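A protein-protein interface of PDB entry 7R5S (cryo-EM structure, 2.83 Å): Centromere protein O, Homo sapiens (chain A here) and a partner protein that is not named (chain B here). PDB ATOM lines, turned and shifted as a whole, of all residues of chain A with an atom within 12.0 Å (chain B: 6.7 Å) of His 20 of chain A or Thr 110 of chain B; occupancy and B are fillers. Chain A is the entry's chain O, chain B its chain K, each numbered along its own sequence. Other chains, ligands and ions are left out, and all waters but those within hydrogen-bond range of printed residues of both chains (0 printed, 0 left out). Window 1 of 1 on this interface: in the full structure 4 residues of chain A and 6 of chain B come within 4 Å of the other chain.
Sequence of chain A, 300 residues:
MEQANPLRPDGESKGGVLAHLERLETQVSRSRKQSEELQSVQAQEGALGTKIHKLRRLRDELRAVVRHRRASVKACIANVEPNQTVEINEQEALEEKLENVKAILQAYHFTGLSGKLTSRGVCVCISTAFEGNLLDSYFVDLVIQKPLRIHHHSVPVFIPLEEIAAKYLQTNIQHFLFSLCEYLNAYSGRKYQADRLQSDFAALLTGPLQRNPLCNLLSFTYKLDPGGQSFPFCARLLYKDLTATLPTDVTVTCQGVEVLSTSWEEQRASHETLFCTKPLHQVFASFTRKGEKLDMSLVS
The side-chain hydroxyl of Ser 113 of chain B sits at hydrogen-bond distance from the backbone carbonyl oxygen of Ser 109 of chain B. A ring nitrogen (ND1) of His 20 of chain A is in hydrogen-bond range of the guanidinium group (NH1) of Arg 23 of chain A. OG1 of Thr 110 of chain B is in hydrogen-bond range of O of Val 107 of chain B, at 2.5 Å. The side-chain hydroxyl (OG1) of Thr 110 of chain B sits at hydrogen-bond distance from the backbone carbonyl oxygen (O) of Met 106 of chain B.
Of the printed residues of chain B, Val 17 of chain A touches Lys 114 (3.8 Å). Leu 18 of chain A touches none of the printed residues of chain B. Of the printed residues of chain B, Leu 24 of chain A touches Met 106. Gln 27 of chain A touches none of the printed residues of chain B. No residue of chain A comes within 4 Å of Val 107 of chain B. Thr 110 of chain B touches just one residue of chain A: His 20. No residue of chain A comes within 4 Å of Lys 111 of chain B. No residue of chain A comes within 4 Å of Glu 112 of chain B. Ser 113 of chain B touches just one residue of chain A: His 20. Lys 114 of chain B touches just one residue of chain A: Val 17. The nearest residue of chain B that does not touch His 20 of chain A is Met 106 of chain B (5.2 Å). The nearest residue of chain A that does not touch Thr 110 of chain B is Leu 24 of chain A (4.5 Å).
The side-chain hydroxyl (OG) of Ser 109 of chain B lies within hydrogen-bond range of a ring nitrogen (NE2) of His 20 of chain A.
Of the 12 printed residues of chain A, 3 touch a printed residue of chain B. Hydrophobic or aromatic side chains of chain A that line the printed part of chain B: Val 17, His 20 and Leu 24. Of the 11 printed residues of chain B, 5 touch a printed residue of chain A. Hydrophobic or aromatic side chains of chain B within 4 Å of the printed part of chain A: Met 106.
Among the printed residues, merely in contact across the chains: His 20 of chain A with Thr 110 of chain B (3.6 Å), His 20 of chain A with Ser 113 of chain B (3.8 Å), Val 17 of chain A with Lys 114 of chain B (3.8 Å) and Leu 24 of chain A with Met 106 of chain B (3.9 Å).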
ATOM      1  N   GLY A  16      34.465   6.723 -16.368  1.00  0.00           N
ATOM      2  CA  GLY A  16      34.234   7.690 -17.425  1.00  0.00           C
ATOM      3  C   GLY A  16      32.955   7.443 -18.199  1.00  0.00           C
ATOM      4  O   GLY A  16      32.166   6.567 -17.848  1.00  0.00           O
ATOM      5  N   VAL A  17      32.749   8.223 -19.260  1.00  0.00           N
ATOM      6  CA  VAL A  17      31.548   8.066 -20.074  1.00  0.00           C
ATOM      7  C   VAL A  17      31.693   6.889 -21.031  1.00  0.00           C
ATOM      8  O   VAL A  17      30.731   6.154 -21.277  1.00  0.00           O
ATOM      9  CB  VAL A  17      31.242   9.375 -20.825  1.00  0.00           C
ATOM     10  CG1 VAL A  17      29.923   9.263 -21.574  1.00  0.00           C
ATOM     11  CG2 VAL A  17      31.212  10.545 -19.856  1.00  0.00           C
ATOM     12  N   LEU A  18      32.894   6.685 -21.577  1.00  0.00           N
ATOM     13  CA  LEU A  18      33.102   5.579 -22.506  1.00  0.00           C
ATOM     14  C   LEU A  18      33.000   4.234 -21.799  1.00  0.00           C
ATOM     15  O   LEU A  18      32.402   3.291 -22.329  1.00  0.00           O
ATOM     16  CB  LEU A  18      34.457   5.724 -23.199  1.00  0.00           C
ATOM     17  CG  LEU A  18      34.648   6.983 -24.048  1.00  0.00           C
ATOM     18  CD1 LEU A  18      36.023   6.995 -24.691  1.00  0.00           C
ATOM     19  CD2 LEU A  18      33.560   7.088 -25.103  1.00  0.00           C
ATOM     20  N   ALA A  19      33.570   4.128 -20.595  1.00  0.00           N
ATOM     21  CA  ALA A  19      33.446   2.890 -19.831  1.00  0.00           C
ATOM     22  C   ALA A  19      31.997   2.630 -19.437  1.00  0.00           C
ATOM     23  O   ALA A  19      31.551   1.477 -19.409  1.00  0.00           O
ATOM     24  CB  ALA A  19      34.340   2.945 -18.595  1.00  0.00           C
ATOM     25  N   HIS A  20      31.243   3.691 -19.140  1.00  0.00           N
ATOM     26  CA  HIS A  20      29.833   3.518 -18.813  1.00  0.00           C
ATOM     27  C   HIS A  20      29.038   3.054 -20.027  1.00  0.00           C
ATOM     28  O   HIS A  20      28.161   2.193 -19.909  1.00  0.00           O
ATOM     29  CB  HIS A  20      29.255   4.817 -18.254  1.00  0.00           C
ATOM     30  CG  HIS A  20      27.932   4.642 -17.579  1.00  0.00           C
ATOM     31  ND1 HIS A  20      27.772   3.875 -16.446  1.00  0.00           N
ATOM     32  CD2 HIS A  20      26.705   5.128 -17.881  1.00  0.00           C
ATOM     33  CE1 HIS A  20      26.505   3.897 -16.077  1.00  0.00           C
ATOM     34  NE2 HIS A  20      25.836   4.652 -16.930  1.00  0.00           N
ATOM     35  N   LEU A  21      29.334   3.611 -21.205  1.00  0.00           N
ATOM     36  CA  LEU A  21      28.687   3.133 -22.422  1.00  0.00           C
ATOM     37  C   LEU A  21      29.039   1.675 -22.690  1.00  0.00           C
ATOM     38  O   LEU A  21      28.184   0.888 -23.112  1.00  0.00           O
ATOM     39  CB  LEU A  21      29.082   4.012 -23.609  1.00  0.00           C
ATOM     40  CG  LEU A  21      28.512   5.431 -23.621  1.00  0.00           C
ATOM     41  CD1 LEU A  21      29.072   6.226 -24.788  1.00  0.00           C
ATOM     42  CD2 LEU A  21      26.994   5.395 -23.676  1.00  0.00           C
ATOM     43  N   GLU A  22      30.291   1.293 -22.429  1.00  0.00           N
ATOM     44  CA  GLU A  22      30.689  -0.101 -22.598  1.00  0.00           C
ATOM     45  C   GLU A  22      29.895  -1.015 -21.673  1.00  0.00           C
ATOM     46  O   GLU A  22      29.324  -2.021 -22.114  1.00  0.00           O
ATOM     47  CB  GLU A  22      32.189  -0.255 -22.344  1.00  0.00           C
ATOM     48  CG  GLU A  22      33.070   0.290 -23.450  1.00  0.00           C
ATOM     49  CD  GLU A  22      34.331  -0.528 -23.641  1.00  0.00           C
ATOM     50  OE1 GLU A  22      34.242  -1.773 -23.611  1.00  0.00           O
ATOM     51  OE2 GLU A  22      35.411   0.073 -23.818  1.00  0.00           O
ATOM     52  N   ARG A  23      29.840  -0.677 -20.382  1.00  0.00           N
ATOM     53  CA  ARG A  23      29.134  -1.526 -19.429  1.00  0.00           C
ATOM     54  C   ARG A  23      27.626  -1.516 -19.649  1.00  0.00           C
ATOM     55  O   ARG A  23      26.948  -2.463 -19.238  1.00  0.00           O
ATOM     56  CB  ARG A  23      29.464  -1.110 -17.992  1.00  0.00           C
ATOM     57  CG  ARG A  23      28.855   0.205 -17.549  1.00  0.00           C
ATOM     58  CD  ARG A  23      29.081   0.435 -16.063  1.00  0.00           C
ATOM     59  NE  ARG A  23      30.501   0.447 -15.721  1.00  0.00           N
ATOM     60  CZ  ARG A  23      31.206   1.551 -15.491  1.00  0.00           C
ATOM     61  NH1 ARG A  23      30.623   2.739 -15.562  1.00  0.00           N
ATOM     62  NH2 ARG A  23      32.494   1.466 -15.188  1.00  0.00           N
ATOM     63  N   LEU A  24      27.086  -0.474 -20.286  1.00  0.00           N
ATOM     64  CA  LEU A  24      25.685  -0.512 -20.693  1.00  0.00           C
ATOM     65  C   LEU A  24      25.495  -1.408 -21.910  1.00  0.00           C
ATOM     66  O   LEU A  24      24.451  -2.053 -22.059  1.00  0.00           O
ATOM     67  CB  LEU A  24      25.180   0.900 -20.986  1.00  0.00           C
ATOM     68  CG  LEU A  24      24.884   1.797 -19.783  1.00  0.00           C
ATOM     69  CD1 LEU A  24      24.470   3.185 -20.245  1.00  0.00           C
ATOM     70  CD2 LEU A  24      23.806   1.179 -18.910  1.00  0.00           C
ATOM     71  N   GLU A  25      26.494  -1.455 -22.795  1.00  0.00           N
ATOM     72  CA  GLU A  25      26.420  -2.335 -23.955  1.00  0.00           C
ATOM     73  C   GLU A  25      26.526  -3.803 -23.559  1.00  0.00           C
ATOM     74  O   GLU A  25      25.868  -4.655 -24.169  1.00  0.00           O
ATOM     75  CB  GLU A  25      27.518  -1.966 -24.955  1.00  0.00           C
ATOM     76  CG  GLU A  25      27.861  -3.053 -25.965  1.00  0.00           C
ATOM     77  CD  GLU A  25      26.785  -3.243 -27.015  1.00  0.00           C
ATOM     78  OE1 GLU A  25      25.915  -2.357 -27.149  1.00  0.00           O
ATOM     79  OE2 GLU A  25      26.810  -4.280 -27.710  1.00  0.00           O
ATOM     80  N   THR A  26      27.335  -4.118 -22.542  1.00  0.00           N
ATOM     81  CA  THR A  26      27.512  -5.512 -22.143  1.00  0.00           C
ATOM     82  C   THR A  26      26.203  -6.129 -21.664  1.00  0.00           C
ATOM     83  O   THR A  26      25.887  -7.274 -22.010  1.00  0.00           O
ATOM     84  CB  THR A  26      28.578  -5.628 -21.053  1.00  0.00           C
ATOM     85  OG1 THR A  26      28.118  -4.988 -19.856  1.00  0.00           O
ATOM     86  CG2 THR A  26      29.889  -5.005 -21.505  1.00  0.00           C
ATOM     87  N   GLN A  27      25.432  -5.393 -20.871  1.00  0.00           N
ATOM     88  CA  GLN A  27      24.166  -5.908 -20.362  1.00  0.00           C
ATOM     89  C   GLN A  27      23.136  -6.009 -21.483  1.00  0.00           C
ATOM     90  O   GLN A  27      22.047  -6.547 -21.290  1.00  0.00           O
ATOM     91  CB  GLN A  27      23.637  -5.023 -19.230  1.00  0.00           C
ATOM     92  CG  GLN A  27      23.023  -3.710 -19.689  1.00  0.00           C
ATOM     93  CD  GLN A  27      21.516  -3.793 -19.849  1.00  0.00           C
ATOM     94  OE1 GLN A  27      20.874  -4.699 -19.318  1.00  0.00           O
ATOM     95  NE2 GLN A  27      20.946  -2.847 -20.586  1.00  0.00           N
ATOM     96  N   GLU B 105      16.312   7.956 -17.617  1.00  0.00           N
ATOM     97  CA  GLU B 105      17.102   7.364 -16.538  1.00  0.00           C
ATOM     98  C   GLU B 105      18.520   7.035 -17.007  1.00  0.00           C
ATOM     99  O   GLU B 105      19.498   7.262 -16.274  1.00  0.00           O
ATOM    100  CB  GLU B 105      16.394   6.130 -15.967  1.00  0.00           C
ATOM    101  CG  GLU B 105      16.573   4.835 -16.738  1.00  0.00           C
ATOM    102  CD  GLU B 105      15.719   3.709 -16.189  1.00  0.00           C
ATOM    103  OE1 GLU B 105      14.877   3.978 -15.306  1.00  0.00           O
ATOM    104  OE2 GLU B 105      15.888   2.557 -16.640  1.00  0.00           O
ATOM    105  N   MET B 106      18.660   6.543 -18.244  1.00  0.00           N
ATOM    106  CA  MET B 106      19.996   6.282 -18.776  1.00  0.00           C
ATOM    107  C   MET B 106      20.787   7.576 -18.939  1.00  0.00           C
ATOM    108  O   MET B 106      21.985   7.630 -18.616  1.00  0.00           O
ATOM    109  CB  MET B 106      19.896   5.538 -20.108  1.00  0.00           C
ATOM    110  CG  MET B 106      19.253   4.165 -20.002  1.00  0.00           C
ATOM    111  SD  MET B 106      19.174   3.301 -21.583  1.00  0.00           S
ATOM    112  CE  MET B 106      20.914   3.111 -21.953  1.00  0.00           C
ATOM    113  N   VAL B 107      20.133   8.628 -19.440  1.00  0.00           N
ATOM    114  CA  VAL B 107      20.800   9.923 -19.574  1.00  0.00           C
ATOM    115  C   VAL B 107      21.284  10.418 -18.215  1.00  0.00           C
ATOM    116  O   VAL B 107      22.396  10.950 -18.090  1.00  0.00           O
ATOM    117  CB  VAL B 107      19.859  10.939 -20.249  1.00  0.00           C
ATOM    118  CG1 VAL B 107      20.433  12.342 -20.158  1.00  0.00           C
ATOM    119  CG2 VAL B 107      19.621  10.555 -21.699  1.00  0.00           C
ATOM    120  N   LEU B 108      20.462  10.243 -17.178  1.00  0.00           N
ATOM    121  CA  LEU B 108      20.839  10.690 -15.839  1.00  0.00           C
ATOM    122  C   LEU B 108      22.068   9.943 -15.334  1.00  0.00           C
ATOM    123  O   LEU B 108      22.993  10.548 -14.772  1.00  0.00           O
ATOM    124  CB  LEU B 108      19.658  10.506 -14.883  1.00  0.00           C
ATOM    125  CG  LEU B 108      19.894  10.695 -13.384  1.00  0.00           C
ATOM    126  CD1 LEU B 108      18.754  11.485 -12.776  1.00  0.00           C
ATOM    127  CD2 LEU B 108      20.033   9.351 -12.685  1.00  0.00           C
ATOM    128  N   SER B 109      22.088   8.620 -15.513  1.00  0.00           N
ATOM    129  CA  SER B 109      23.249   7.842 -15.087  1.00  0.00           C
ATOM    130  C   SER B 109      24.517   8.307 -15.803  1.00  0.00           C
ATOM    131  O   SER B 109      25.581   8.475 -15.179  1.00  0.00           O
ATOM    132  CB  SER B 109      22.998   6.356 -15.338  1.00  0.00           C
ATOM    133  OG  SER B 109      24.215   5.638 -15.393  1.00  0.00           O
ATOM    134  N   THR B 110      24.420   8.528 -17.118  1.00  0.00           N
ATOM    135  CA  THR B 110      25.584   8.985 -17.872  1.00  0.00           C
ATOM    136  C   THR B 110      26.058  10.353 -17.389  1.00  0.00           C
ATOM    137  O   THR B 110      27.267  10.599 -17.287  1.00  0.00           O
ATOM    138  CB  THR B 110      25.267   9.027 -19.367  1.00  0.00           C
ATOM    139  OG1 THR B 110      24.118   9.854 -19.591  1.00  0.00           O
ATOM    140  CG2 THR B 110      24.990   7.626 -19.891  1.00  0.00           C
ATOM    141  N   LYS B 111      25.119  11.255 -17.087  1.00  0.00           N
ATOM    142  CA  LYS B 111      25.499  12.577 -16.594  1.00  0.00           C
ATOM    143  C   LYS B 111      26.212  12.484 -15.250  1.00  0.00           C
ATOM    144  O   LYS B 111      27.178  13.218 -14.997  1.00  0.00           O
ATOM    145  CB  LYS B 111      24.266  13.474 -16.486  1.00  0.00           C
ATOM    146  CG  LYS B 111      23.638  13.841 -17.821  1.00  0.00           C
ATOM    147  CD  LYS B 111      24.564  14.711 -18.653  1.00  0.00           C
ATOM    148  CE  LYS B 111      24.813  16.051 -17.982  1.00  0.00           C
ATOM    149  NZ  LYS B 111      25.673  16.938 -18.815  1.00  0.00           N
ATOM    150  N   GLU B 112      25.749  11.590 -14.374  1.00  0.00           N
ATOM    151  CA  GLU B 112      26.421  11.404 -13.089  1.00  0.00           C
ATOM    152  C   GLU B 112      27.860  10.934 -13.285  1.00  0.00           C
ATOM    153  O   GLU B 112      28.795  11.462 -12.660  1.00  0.00           O
ATOM    154  CB  GLU B 112      25.643  10.408 -12.229  1.00  0.00           C
ATOM    155  CG  GLU B 112      24.269  10.893 -11.803  1.00  0.00           C
ATOM    156  CD  GLU B 112      23.476   9.826 -11.077  1.00  0.00           C
ATOM    157  OE1 GLU B 112      23.889   8.647 -11.113  1.00  0.00           O
ATOM    158  OE2 GLU B 112      22.440  10.164 -10.468  1.00  0.00           O
ATOM    159  N   SER B 113      28.052   9.931 -14.150  1.00  0.00           N
ATOM    160  CA  SER B 113      29.408   9.457 -14.424  1.00  0.00           C
ATOM    161  C   SER B 113      30.286  10.577 -14.978  1.00  0.00           C
ATOM    162  O   SER B 113      31.454  10.725 -14.583  1.00  0.00           O
ATOM    163  CB  SER B 113      29.364   8.279 -15.397  1.00  0.00           C
ATOM    164  OG  SER B 113      28.676   7.178 -14.834  1.00  0.00           O
ATOM    165  N   LYS B 114      29.734  11.374 -15.897  1.00  0.00           N
ATOM    166  CA  LYS B 114      30.481  12.488 -16.473  1.00  0.00           C
ATOM    167  C   LYS B 114      30.912  13.482 -15.402  1.00  0.00           C
ATOM    168  O   LYS B 114      32.057  13.951 -15.405  1.00  0.00           O
ATOM    169  CB  LYS B 114      29.635  13.178 -17.543  1.00  0.00           C
ATOM    170  CG  LYS B 114      30.270  14.413 -18.157  1.00  0.00           C
ATOM    171  CD  LYS B 114      29.380  14.991 -19.245  1.00  0.00           C
ATOM    172  CE  LYS B 114      30.019  16.202 -19.905  1.00  0.00           C
ATOM    173  NZ  LYS B 114      30.188  17.330 -18.952  1.00  0.00           N
ATOM    174  N   ASN B 115      30.008  13.816 -14.478  1.00  0.00           N
ATOM    175  CA  ASN B 115      30.348  14.767 -13.422  1.00  0.00           C
ATOM    176  C   ASN B 115      31.457  14.231 -12.524  1.00  0.00           C
ATOM    177  O   ASN B 115      32.377  14.973 -12.146  1.00  0.00           O
ATOM    178  CB  ASN B 115      29.107  15.103 -12.597  1.00  0.00           C
ATOM    179  CG  ASN B 115      28.222  16.131 -13.269  1.00  0.00           C
ATOM    180  OD1 ASN B 115      28.334  16.372 -14.471  1.00  0.00           O
ATOM    181  ND2 ASN B 115      27.336  16.746 -12.496  1.00  0.00           N
